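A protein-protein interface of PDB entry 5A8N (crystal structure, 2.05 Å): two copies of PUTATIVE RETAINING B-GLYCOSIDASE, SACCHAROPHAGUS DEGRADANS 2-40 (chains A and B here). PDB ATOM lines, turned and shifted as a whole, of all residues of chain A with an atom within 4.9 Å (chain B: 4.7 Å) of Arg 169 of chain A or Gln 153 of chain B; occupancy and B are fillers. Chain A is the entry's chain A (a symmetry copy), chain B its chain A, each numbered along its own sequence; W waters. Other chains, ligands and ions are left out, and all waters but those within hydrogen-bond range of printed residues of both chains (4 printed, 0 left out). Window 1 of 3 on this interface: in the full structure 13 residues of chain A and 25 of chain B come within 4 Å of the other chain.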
ATOM      1  N   TYR A  36     -28.760   4.553  17.495  1.00  0.00           N
ATOM      2  CA  TYR A  36     -27.494   3.998  17.027  1.00  0.00           C
ATOM      3  C   TYR A  36     -26.912   3.102  18.135  1.00  0.00           C
ATOM      4  O   TYR A  36     -27.142   3.363  19.336  1.00  0.00           O
ATOM      5  CB  TYR A  36     -26.526   5.133  16.664  1.00  0.00           C
ATOM      6  CG  TYR A  36     -26.817   5.716  15.308  1.00  0.00           C
ATOM      7  CD1 TYR A  36     -27.785   6.723  15.130  1.00  0.00           C
ATOM      8  CD2 TYR A  36     -26.150   5.244  14.187  1.00  0.00           C
ATOM      9  CE1 TYR A  36     -28.063   7.232  13.854  1.00  0.00           C
ATOM     10  CE2 TYR A  36     -26.400   5.748  12.935  1.00  0.00           C
ATOM     11  CZ  TYR A  36     -27.355   6.739  12.759  1.00  0.00           C
ATOM     12  OH  TYR A  36     -27.587   7.208  11.475  1.00  0.00           O
ATOM     13  N   ARG A 165     -21.832 -10.657   7.142  1.00  0.00           N
ATOM     14  CA  ARG A 165     -21.115  -9.388   7.266  1.00  0.00           C
ATOM     15  C   ARG A 165     -21.671  -8.559   8.416  1.00  0.00           C
ATOM     16  O   ARG A 165     -20.929  -8.005   9.220  1.00  0.00           O
ATOM     17  CB  ARG A 165     -21.249  -8.583   5.983  1.00  0.00           C
ATOM     18  CG  ARG A 165     -20.481  -9.138   4.791  1.00  0.00           C
ATOM     19  CD  ARG A 165     -20.555  -8.139   3.640  1.00  0.00           C
ATOM     20  NE  ARG A 165     -19.960  -8.631   2.415  1.00  0.00           N
ATOM     21  CZ  ARG A 165     -18.668  -8.613   2.146  1.00  0.00           C
ATOM     22  NH1 ARG A 165     -17.813  -8.163   3.043  1.00  0.00           N
ATOM     23  NH2 ARG A 165     -18.228  -9.062   0.980  1.00  0.00           N
ATOM     24  N   ASP A 166     -22.991  -8.465   8.475  1.00  0.00           N
ATOM     25  CA  ASP A 166     -23.645  -7.683   9.502  1.00  0.00           C
ATOM     26  C   ASP A 166     -23.310  -8.201  10.903  1.00  0.00           C
ATOM     27  O   ASP A 166     -23.041  -7.410  11.811  1.00  0.00           O
ATOM     28  CB  ASP A 166     -25.146  -7.685   9.294  1.00  0.00           C
ATOM     29  CG  ASP A 166     -25.867  -6.903  10.373  1.00  0.00           C
ATOM     30  OD1 ASP A 166     -25.602  -5.670  10.508  1.00  0.00           O
ATOM     31  OD2 ASP A 166     -26.649  -7.525  11.113  1.00  0.00           O
ATOM     32  N   PHE A 167     -23.322  -9.516  11.076  1.00  0.00           N
ATOM     33  CA  PHE A 167     -22.935 -10.118  12.359  1.00  0.00           C
ATOM     34  C   PHE A 167     -21.540  -9.647  12.758  1.00  0.00           C
ATOM     35  O   PHE A 167     -21.336  -9.182  13.884  1.00  0.00           O
ATOM     36  CB  PHE A 167     -22.980 -11.653  12.276  1.00  0.00           C
ATOM     37  CG  PHE A 167     -22.405 -12.358  13.492  1.00  0.00           C
ATOM     38  CD1 PHE A 167     -23.126 -12.466  14.671  1.00  0.00           C
ATOM     39  CD2 PHE A 167     -21.145 -12.918  13.437  1.00  0.00           C
ATOM     40  CE1 PHE A 167     -22.603 -13.101  15.772  1.00  0.00           C
ATOM     41  CE2 PHE A 167     -20.611 -13.553  14.532  1.00  0.00           C
ATOM     42  CZ  PHE A 167     -21.341 -13.651  15.713  1.00  0.00           C
ATOM     43  N   TRP A 168     -20.578  -9.737  11.838  1.00  0.00           N
ATOM     44  CA  TRP A 168     -19.201  -9.376  12.202  1.00  0.00           C
ATOM     45  C   TRP A 168     -19.055  -7.856  12.382  1.00  0.00           C
ATOM     46  O   TRP A 168     -18.293  -7.377  13.235  1.00  0.00           O
ATOM     47  CB  TRP A 168     -18.173  -9.965  11.216  1.00  0.00           C
ATOM     48  CG  TRP A 168     -18.028 -11.431  11.397  1.00  0.00           C
ATOM     49  CD1 TRP A 168     -18.295 -12.410  10.484  1.00  0.00           C
ATOM     50  CD2 TRP A 168     -17.645 -12.101  12.602  1.00  0.00           C
ATOM     51  NE1 TRP A 168     -18.089 -13.648  11.049  1.00  0.00           N
ATOM     52  CE2 TRP A 168     -17.691 -13.485  12.345  1.00  0.00           C
ATOM     53  CE3 TRP A 168     -17.244 -11.665  13.863  1.00  0.00           C
ATOM     54  CZ2 TRP A 168     -17.377 -14.433  13.304  1.00  0.00           C
ATOM     55  CZ3 TRP A 168     -16.921 -12.622  14.832  1.00  0.00           C
ATOM     56  CH2 TRP A 168     -16.976 -13.981  14.543  1.00  0.00           C
ATOM     57  N   ARG A 169     -19.818  -7.083  11.616  1.00  0.00           N
ATOM     58  CA  ARG A 169     -19.779  -5.635  11.781  1.00  0.00           C
ATOM     59  C   ARG A 169     -20.269  -5.266  13.196  1.00  0.00           C
ATOM     60  O   ARG A 169     -19.653  -4.464  13.879  1.00  0.00           O
ATOM     61  CB  ARG A 169     -20.618  -4.945  10.691  1.00  0.00           C
ATOM     62  CG  ARG A 169     -20.741  -3.431  10.810  1.00  0.00           C
ATOM     63  CD  ARG A 169     -21.886  -2.992  11.730  1.00  0.00           C
ATOM     64  NE  ARG A 169     -22.099  -1.531  11.648  1.00  0.00           N
ATOM     65  CZ  ARG A 169     -22.863  -0.913  10.752  1.00  0.00           C
ATOM     66  NH1 ARG A 169     -23.511  -1.602   9.825  1.00  0.00           N
ATOM     67  NH2 ARG A 169     -22.975   0.414  10.776  1.00  0.00           N
ATOM     68  N   ARG A 170     -21.387  -5.857  13.611  1.00  0.00           N
ATOM     69  CA  ARG A 170     -21.965  -5.585  14.924  1.00  0.00           C
ATOM     70  C   ARG A 170     -21.068  -6.065  16.056  1.00  0.00           C
ATOM     71  O   ARG A 170     -20.883  -5.355  17.030  1.00  0.00           O
ATOM     72  CB  ARG A 170     -23.294  -6.306  15.068  1.00  0.00           C
ATOM     73  CG  ARG A 170     -24.461  -5.722  14.295  1.00  0.00           C
ATOM     74  CD  ARG A 170     -25.615  -6.685  14.492  1.00  0.00           C
ATOM     75  NE  ARG A 170     -26.818  -6.393  13.726  1.00  0.00           N
ATOM     76  CZ  ARG A 170     -27.841  -5.690  14.182  1.00  0.00           C
ATOM     77  NH1 ARG A 170     -27.811  -5.151  15.382  1.00  0.00           N
ATOM     78  NH2 ARG A 170     -28.910  -5.525  13.421  1.00  0.00           N
ATOM     79  N   ILE A 171     -20.522  -7.278  15.918  1.00  0.00           N
ATOM     80  CA  ILE A 171     -19.659  -7.874  16.928  1.00  0.00           C
ATOM     81  C   ILE A 171     -18.370  -7.069  17.092  1.00  0.00           C
ATOM     82  O   ILE A 171     -17.970  -6.766  18.206  1.00  0.00           O
ATOM     83  CB  ILE A 171     -19.325  -9.334  16.582  1.00  0.00           C
ATOM     84  CG1 ILE A 171     -20.555 -10.224  16.747  1.00  0.00           C
ATOM     85  CG2 ILE A 171     -18.140  -9.859  17.396  1.00  0.00           C
ATOM     86  CD1 ILE A 171     -20.848 -10.590  18.175  1.00  0.00           C
ATOM     87  N   THR A 172     -17.739  -6.700  15.985  1.00  0.00           N
ATOM     88  CA  THR A 172     -16.463  -6.014  16.066  1.00  0.00           C
ATOM     89  C   THR A 172     -16.602  -4.596  16.686  1.00  0.00           C
ATOM     90  O   THR A 172     -15.768  -4.169  17.500  1.00  0.00           O
ATOM     91  CB  THR A 172     -15.802  -5.910  14.691  1.00  0.00           C
ATOM     92  OG1 THR A 172     -15.739  -7.209  14.089  1.00  0.00           O
ATOM     93  CG2 THR A 172     -14.379  -5.349  14.840  1.00  0.00           C
ATOM     94  N   PHE A 173     -17.654  -3.879  16.305  1.00  0.00           N
ATOM     95  CA  PHE A 173     -17.944  -2.589  16.904  1.00  0.00           C
ATOM     96  C   PHE A 173     -18.209  -2.737  18.403  1.00  0.00           C
ATOM     97  O   PHE A 173     -17.661  -2.002  19.215  1.00  0.00           O
ATOM     98  CB  PHE A 173     -19.173  -1.951  16.225  1.00  0.00           C
ATOM     99  CG  PHE A 173     -19.623  -0.667  16.855  1.00  0.00           C
ATOM    100  CD1 PHE A 173     -18.918   0.520  16.629  1.00  0.00           C
ATOM    101  CD2 PHE A 173     -20.750  -0.635  17.670  1.00  0.00           C
ATOM    102  CE1 PHE A 173     -19.337   1.718  17.210  1.00  0.00           C
ATOM    103  CE2 PHE A 173     -21.182   0.560  18.242  1.00  0.00           C
ATOM    104  CZ  PHE A 173     -20.473   1.729  18.010  1.00  0.00           C
ATOM    105  N   MET A 215     -13.211  -5.850   6.902  1.00  0.00           N
ATOM    106  CA  MET A 215     -14.273  -5.169   7.686  1.00  0.00           C
ATOM    107  C   MET A 215     -13.927  -5.172   9.164  1.00  0.00           C
ATOM    108  O   MET A 215     -14.148  -4.179   9.881  1.00  0.00           O
ATOM    109  CB  MET A 215     -15.633  -5.860   7.552  1.00  0.00           C
ATOM    110  CG  MET A 215     -16.342  -5.692   6.239  1.00  0.00           C
ATOM    111  SD  MET A 215     -17.908  -6.618   6.289  1.00  0.00           S
ATOM    112  CE  MET A 215     -18.922  -5.455   7.194  1.00  0.00           C
ATOM    113  N   ILE B 144     -27.923   5.197   3.343  1.00  0.00           N
ATOM    114  CA  ILE B 144     -26.573   5.647   3.701  1.00  0.00           C
ATOM    115  C   ILE B 144     -25.752   4.390   3.978  1.00  0.00           C
ATOM    116  O   ILE B 144     -26.093   3.604   4.853  1.00  0.00           O
ATOM    117  CB  ILE B 144     -26.562   6.560   4.966  1.00  0.00           C
ATOM    118  CG1 ILE B 144     -27.517   7.738   4.767  1.00  0.00           C
ATOM    119  CG2 ILE B 144     -25.133   7.057   5.254  1.00  0.00           C
ATOM    120  CD1 ILE B 144     -27.534   8.783   5.890  1.00  0.00           C
ATOM    121  N   GLY B 145     -24.710   4.168   3.191  1.00  0.00           N
ATOM    122  CA  GLY B 145     -23.900   2.976   3.320  1.00  0.00           C
ATOM    123  C   GLY B 145     -23.355   2.507   2.002  1.00  0.00           C
ATOM    124  O   GLY B 145     -23.190   3.295   1.049  1.00  0.00           O
ATOM    125  N   GLN B 151     -24.345  -3.166   3.375  1.00  0.00           N
ATOM    126  CA  GLN B 151     -24.105  -2.813   4.782  1.00  0.00           C
ATOM    127  C   GLN B 151     -24.326  -1.304   4.911  1.00  0.00           C
ATOM    128  O   GLN B 151     -23.934  -0.536   4.017  1.00  0.00           O
ATOM    129  CB  GLN B 151     -22.682  -3.182   5.229  1.00  0.00           C
ATOM    130  CG  GLN B 151     -22.246  -4.629   5.004  1.00  0.00           C
ATOM    131  CD  GLN B 151     -23.078  -5.633   5.783  1.00  0.00           C
ATOM    132  OE1 GLN B 151     -23.083  -5.620   7.002  1.00  0.00           O
ATOM    133  NE2 GLN B 151     -23.770  -6.517   5.075  1.00  0.00           N
ATOM    134  N   TYR B 152     -24.956  -0.877   6.006  1.00  0.00           N
ATOM    135  CA  TYR B 152     -25.479   0.509   6.112  1.00  0.00           C
ATOM    136  C   TYR B 152     -25.178   1.187   7.445  1.00  0.00           C
ATOM    137  O   TYR B 152     -24.868   0.544   8.444  1.00  0.00           O
ATOM    138  CB  TYR B 152     -26.997   0.518   5.859  1.00  0.00           C
ATOM    139  CG  TYR B 152     -27.293  -0.185   4.582  1.00  0.00           C
ATOM    140  CD1 TYR B 152     -27.131   0.460   3.374  1.00  0.00           C
ATOM    141  CD2 TYR B 152     -27.634  -1.536   4.572  1.00  0.00           C
ATOM    142  CE1 TYR B 152     -27.337  -0.190   2.182  1.00  0.00           C
ATOM    143  CE2 TYR B 152     -27.845  -2.203   3.380  1.00  0.00           C
ATOM    144  CZ  TYR B 152     -27.679  -1.519   2.183  1.00  0.00           C
ATOM    145  OH  TYR B 152     -27.879  -2.141   0.990  1.00  0.00           O
ATOM    146  N   GLN B 153     -25.338   2.492   7.458  1.00  0.00           N
ATOM    147  CA  GLN B 153     -25.075   3.267   8.658  1.00  0.00           C
ATOM    148  C   GLN B 153     -26.095   2.967   9.771  1.00  0.00           C
ATOM    149  O   GLN B 153     -25.771   3.050  10.938  1.00  0.00           O
ATOM    150  CB  GLN B 153     -25.089   4.750   8.308  1.00  0.00           C
ATOM    151  CG  GLN B 153     -24.893   5.653   9.500  1.00  0.00           C
ATOM    152  CD  GLN B 153     -24.614   7.068   9.101  1.00  0.00           C
ATOM    153  OE1 GLN B 153     -23.633   7.339   8.432  1.00  0.00           O
ATOM    154  NE2 GLN B 153     -25.455   7.979   9.535  1.00  0.00           N
ATOM    155  N   HIS B 154     -27.326   2.619   9.408  1.00  0.00           N
ATOM    156  CA  HIS B 154     -28.419   2.447  10.390  1.00  0.00           C
ATOM    157  C   HIS B 154     -29.513   1.615   9.724  1.00  0.00           C
ATOM    158  O   HIS B 154     -29.689   1.685   8.513  1.00  0.00           O
ATOM    159  CB  HIS B 154     -28.961   3.822  10.769  1.00  0.00           C
ATOM    160  CG  HIS B 154     -29.989   3.823  11.853  1.00  0.00           C
ATOM    161  ND1 HIS B 154     -31.307   3.492  11.631  1.00  0.00           N
ATOM    162  CD2 HIS B 154     -29.913   4.192  13.155  1.00  0.00           C
ATOM    163  CE1 HIS B 154     -31.993   3.611  12.755  1.00  0.00           C
ATOM    164  NE2 HIS B 154     -31.170   4.042  13.694  1.00  0.00           N
ATOM    165  N   TYR B 157     -32.006   2.623   6.912  1.00  0.00           N
ATOM    166  CA  TYR B 157     -31.469   2.721   5.547  1.00  0.00           C
ATOM    167  C   TYR B 157     -31.244   1.353   4.895  1.00  0.00           C
ATOM    168  O   TYR B 157     -30.819   1.267   3.734  1.00  0.00           O
ATOM    169  CB  TYR B 157     -30.145   3.478   5.551  1.00  0.00           C
ATOM    170  CG  TYR B 157     -30.181   4.820   6.270  1.00  0.00           C
ATOM    171  CD1 TYR B 157     -31.056   5.820   5.867  1.00  0.00           C
ATOM    172  CD2 TYR B 157     -29.347   5.081   7.344  1.00  0.00           C
ATOM    173  CE1 TYR B 157     -31.108   7.032   6.529  1.00  0.00           C
ATOM    174  CE2 TYR B 157     -29.399   6.288   8.036  1.00  0.00           C
ATOM    175  CZ  TYR B 157     -30.284   7.258   7.614  1.00  0.00           C
ATOM    176  OH  TYR B 157     -30.361   8.467   8.262  1.00  0.00           O
ATOM    177  N   MET B 193     -17.986   4.047   5.787  1.00  0.00           N
ATOM    178  CA  MET B 193     -17.687   4.403   7.180  1.00  0.00           C
ATOM    179  C   MET B 193     -16.297   3.950   7.588  1.00  0.00           C
ATOM    180  O   MET B 193     -16.114   3.125   8.475  1.00  0.00           O
ATOM    181  CB  MET B 193     -18.767   3.847   8.141  1.00  0.00           C
ATOM    182  CG  MET B 193     -20.197   4.333   7.824  1.00  0.00           C
ATOM    183  SD  MET B 193     -21.421   3.689   8.992  1.00  0.00           S
ATOM    184  CE  MET B 193     -21.043   4.676  10.441  1.00  0.00           C
ATOM    185  N   THR B 196     -15.463   0.131   7.328  1.00  0.00           N
ATOM    186  CA  THR B 196     -16.090  -0.809   8.249  1.00  0.00           C
ATOM    187  C   THR B 196     -17.277  -1.499   7.581  1.00  0.00           C
ATOM    188  O   THR B 196     -17.728  -2.543   8.048  1.00  0.00           O
ATOM    189  CB  THR B 196     -16.578  -0.127   9.549  1.00  0.00           C
ATOM    190  OG1 THR B 196     -17.469   0.944   9.237  1.00  0.00           O
ATOM    191  CG2 THR B 196     -15.427   0.439  10.348  1.00  0.00           C
ATOM    192  N   LEU B 197     -17.806  -0.916   6.505  1.00  0.00           N
ATOM    193  CA  LEU B 197     -18.982  -1.481   5.815  1.00  0.00           C
ATOM    194  C   LEU B 197     -18.597  -2.332   4.615  1.00  0.00           C
ATOM    195  O   LEU B 197     -19.439  -3.048   4.075  1.00  0.00           O
ATOM    196  CB  LEU B 197     -19.921  -0.376   5.360  1.00  0.00           C
ATOM    197  CG  LEU B 197     -20.521   0.508   6.455  1.00  0.00           C
ATOM    198  CD1 LEU B 197     -21.570   1.408   5.841  1.00  0.00           C
ATOM    199  CD2 LEU B 197     -21.112  -0.330   7.573  1.00  0.00           C
ATOM    200  N   TRP B 232     -19.940   9.958   1.988  1.00  0.00           N
ATOM    201  CA  TRP B 232     -21.310  10.440   2.123  1.00  0.00           C
ATOM    202  C   TRP B 232     -21.704  11.438   1.011  1.00  0.00           C
ATOM    203  O   TRP B 232     -22.132  12.544   1.297  1.00  0.00           O
ATOM    204  CB  TRP B 232     -21.568  11.057   3.503  1.00  0.00           C
ATOM    205  CG  TRP B 232     -21.568  10.118   4.696  1.00  0.00           C
ATOM    206  CD1 TRP B 232     -22.664   9.613   5.328  1.00  0.00           C
ATOM    207  CD2 TRP B 232     -20.426   9.621   5.423  1.00  0.00           C
ATOM    208  NE1 TRP B 232     -22.278   8.814   6.402  1.00  0.00           N
ATOM    209  CE2 TRP B 232     -20.915   8.805   6.474  1.00  0.00           C
ATOM    210  CE3 TRP B 232     -19.039   9.782   5.287  1.00  0.00           C
ATOM    211  CZ2 TRP B 232     -20.068   8.167   7.383  1.00  0.00           C
ATOM    212  CZ3 TRP B 232     -18.197   9.139   6.181  1.00  0.00           C
ATOM    213  CH2 TRP B 232     -18.715   8.343   7.218  1.00  0.00           C
HETATM  214  O   HOH W   1     -29.582   8.702  11.067  1.00  0.00           O
HETATM  215  O   HOH W   2     -24.004  -4.205   9.069  1.00  0.00           O
HETATM  216  O   HOH W   3     -26.015  -2.823   7.794  1.00  0.00           O
HETATM  217  O   HOH W   4     -16.806  -3.600  10.467  1.00  0.00           O
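The backbone carbonyl oxygen (O) of Tyr 152 of chain B is in hydrogen-bond range of the guanidinium group (NH1) of Arg 169 of chain A, at 2.9 Å. The backbone NH (N) of Asp 166 of chain A is in hydrogen-bond range of the side-chain amide oxygen (OE1) of Gln 151 of chain B, at 3.2 Å. The side-chain hydroxyl (OH) of Tyr 36 of chain A lies within hydrogen-bond range of the side-chain amide nitrogen (NE2) of Gln 153 of chain B (3.0 Å).
The guanidinium group (NH1) of Arg 165 of chain A sits at hydrogen-bond distance from the side-chain sulfur (SD) of Met 215 of chain A. NE of Arg 170 of chain A lies within salt-bridge range of OD2 of Asp 166 of chain A (2.9 Å). The indole nitrogen of Trp 232 of chain B sits at hydrogen-bond distance from the side-chain amide oxygen of Gln 153 of chain B. The backbone carbonyl oxygen (O) of Ile 144 of chain B sits at hydrogen-bond distance from the backbone NH (N) of Gln 153 of chain B (2.9 Å). The backbone carbonyl oxygen of Met 193 of chain B sits at hydrogen-bond distance from the side-chain hydroxyl of Thr 196 of chain B.
Tyr 36 of chain A touches His 154 of chain B. CE2 of Tyr 157 of chain B touches OH of Tyr 36 of chain A, at 3.99 Å. Arg 165 of chain A touches Gln 151 of chain B. NH2 of Arg 169 of chain A touches O of Gln 153 of chain B (3.8 Å). Arg 169 of chain A touches Leu 197 of chain B. CE of Met 215 of chain A touches O of Thr 196 of chain B, 3.3 Å away. Met 215 of chain A touches Leu 197 of chain B.
Printed residues of chain B within 4 Å of Asp 166 of chain A: Gln 151 (3.2 Å). Trp 168 of chain A touches none of the printed residues of chain B. Arg 169 of chain A touches just these residues of chain B: Tyr 152 (2.9 Å), Gln 153 (3.8 Å) and Leu 197 (3.5 Å). Gly 145 of chain B touches none of the printed residues of chain A. Printed residues of chain A within 4 Å of Gln 153 of chain B: Tyr 36 and Arg 169. Printed residues of chain A within 4 Å of Thr 196 of chain B: Met 215 (3.3 Å). The nearest printed residue of chain A that does not touch Gln 153 of chain B is Asp 166 of chain A (8.7 Å). The nearest printed residue of chain A that does not touch Tyr 152 of chain B is Asp 166 of chain A (6.6 Å).
Of the 11 printed residues of chain A, 5 touch a printed residue of chain B. Hydrophobic or aromatic side chains of chain A within 4 Å of the printed part of chain B: Tyr 36 and Met 215. Hydrophobic or aromatic side chains of chain B within 4 Å of the printed part of chain A: His 154, Tyr 157 and Leu 197. Along chain B the printed residues that touch a printed residue of chain A span positions 151 to 197. Among the printed residues, 10 pairs touch across the chains. Among the printed residues, no Asp or Glu carboxylate lies within 4 Å of a Lys or Arg side-chain nitrogen of the other chain.
No position is printed for both chains.
Water W1 lies within hydrogen-bond range of the side-chain hydroxyl of Tyr 36 of chain A and the side-chain hydroxyl of Tyr 157 of chain B. Water W2 lies within hydrogen-bond range of the side-chain carboxylate (OD1) of Asp 166 of chain A (2.6 Å), the side-chain amide oxygen (OE1) of Gln 151 of chain B (2.7 Å) and the guanidinium group (NH1) of Arg 169 of chain A (2.8 Å). Water W4 lies within hydrogen-bond range of O of Met 215 of chain A (2.8 Å) and O of Thr 196 of chain B (2.8 Å). Water W3 bridges the backbone NH of Tyr 152 of chain B (2.8 Å) and the guanidinium group of Arg 169 of chain A (3.4 Å).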
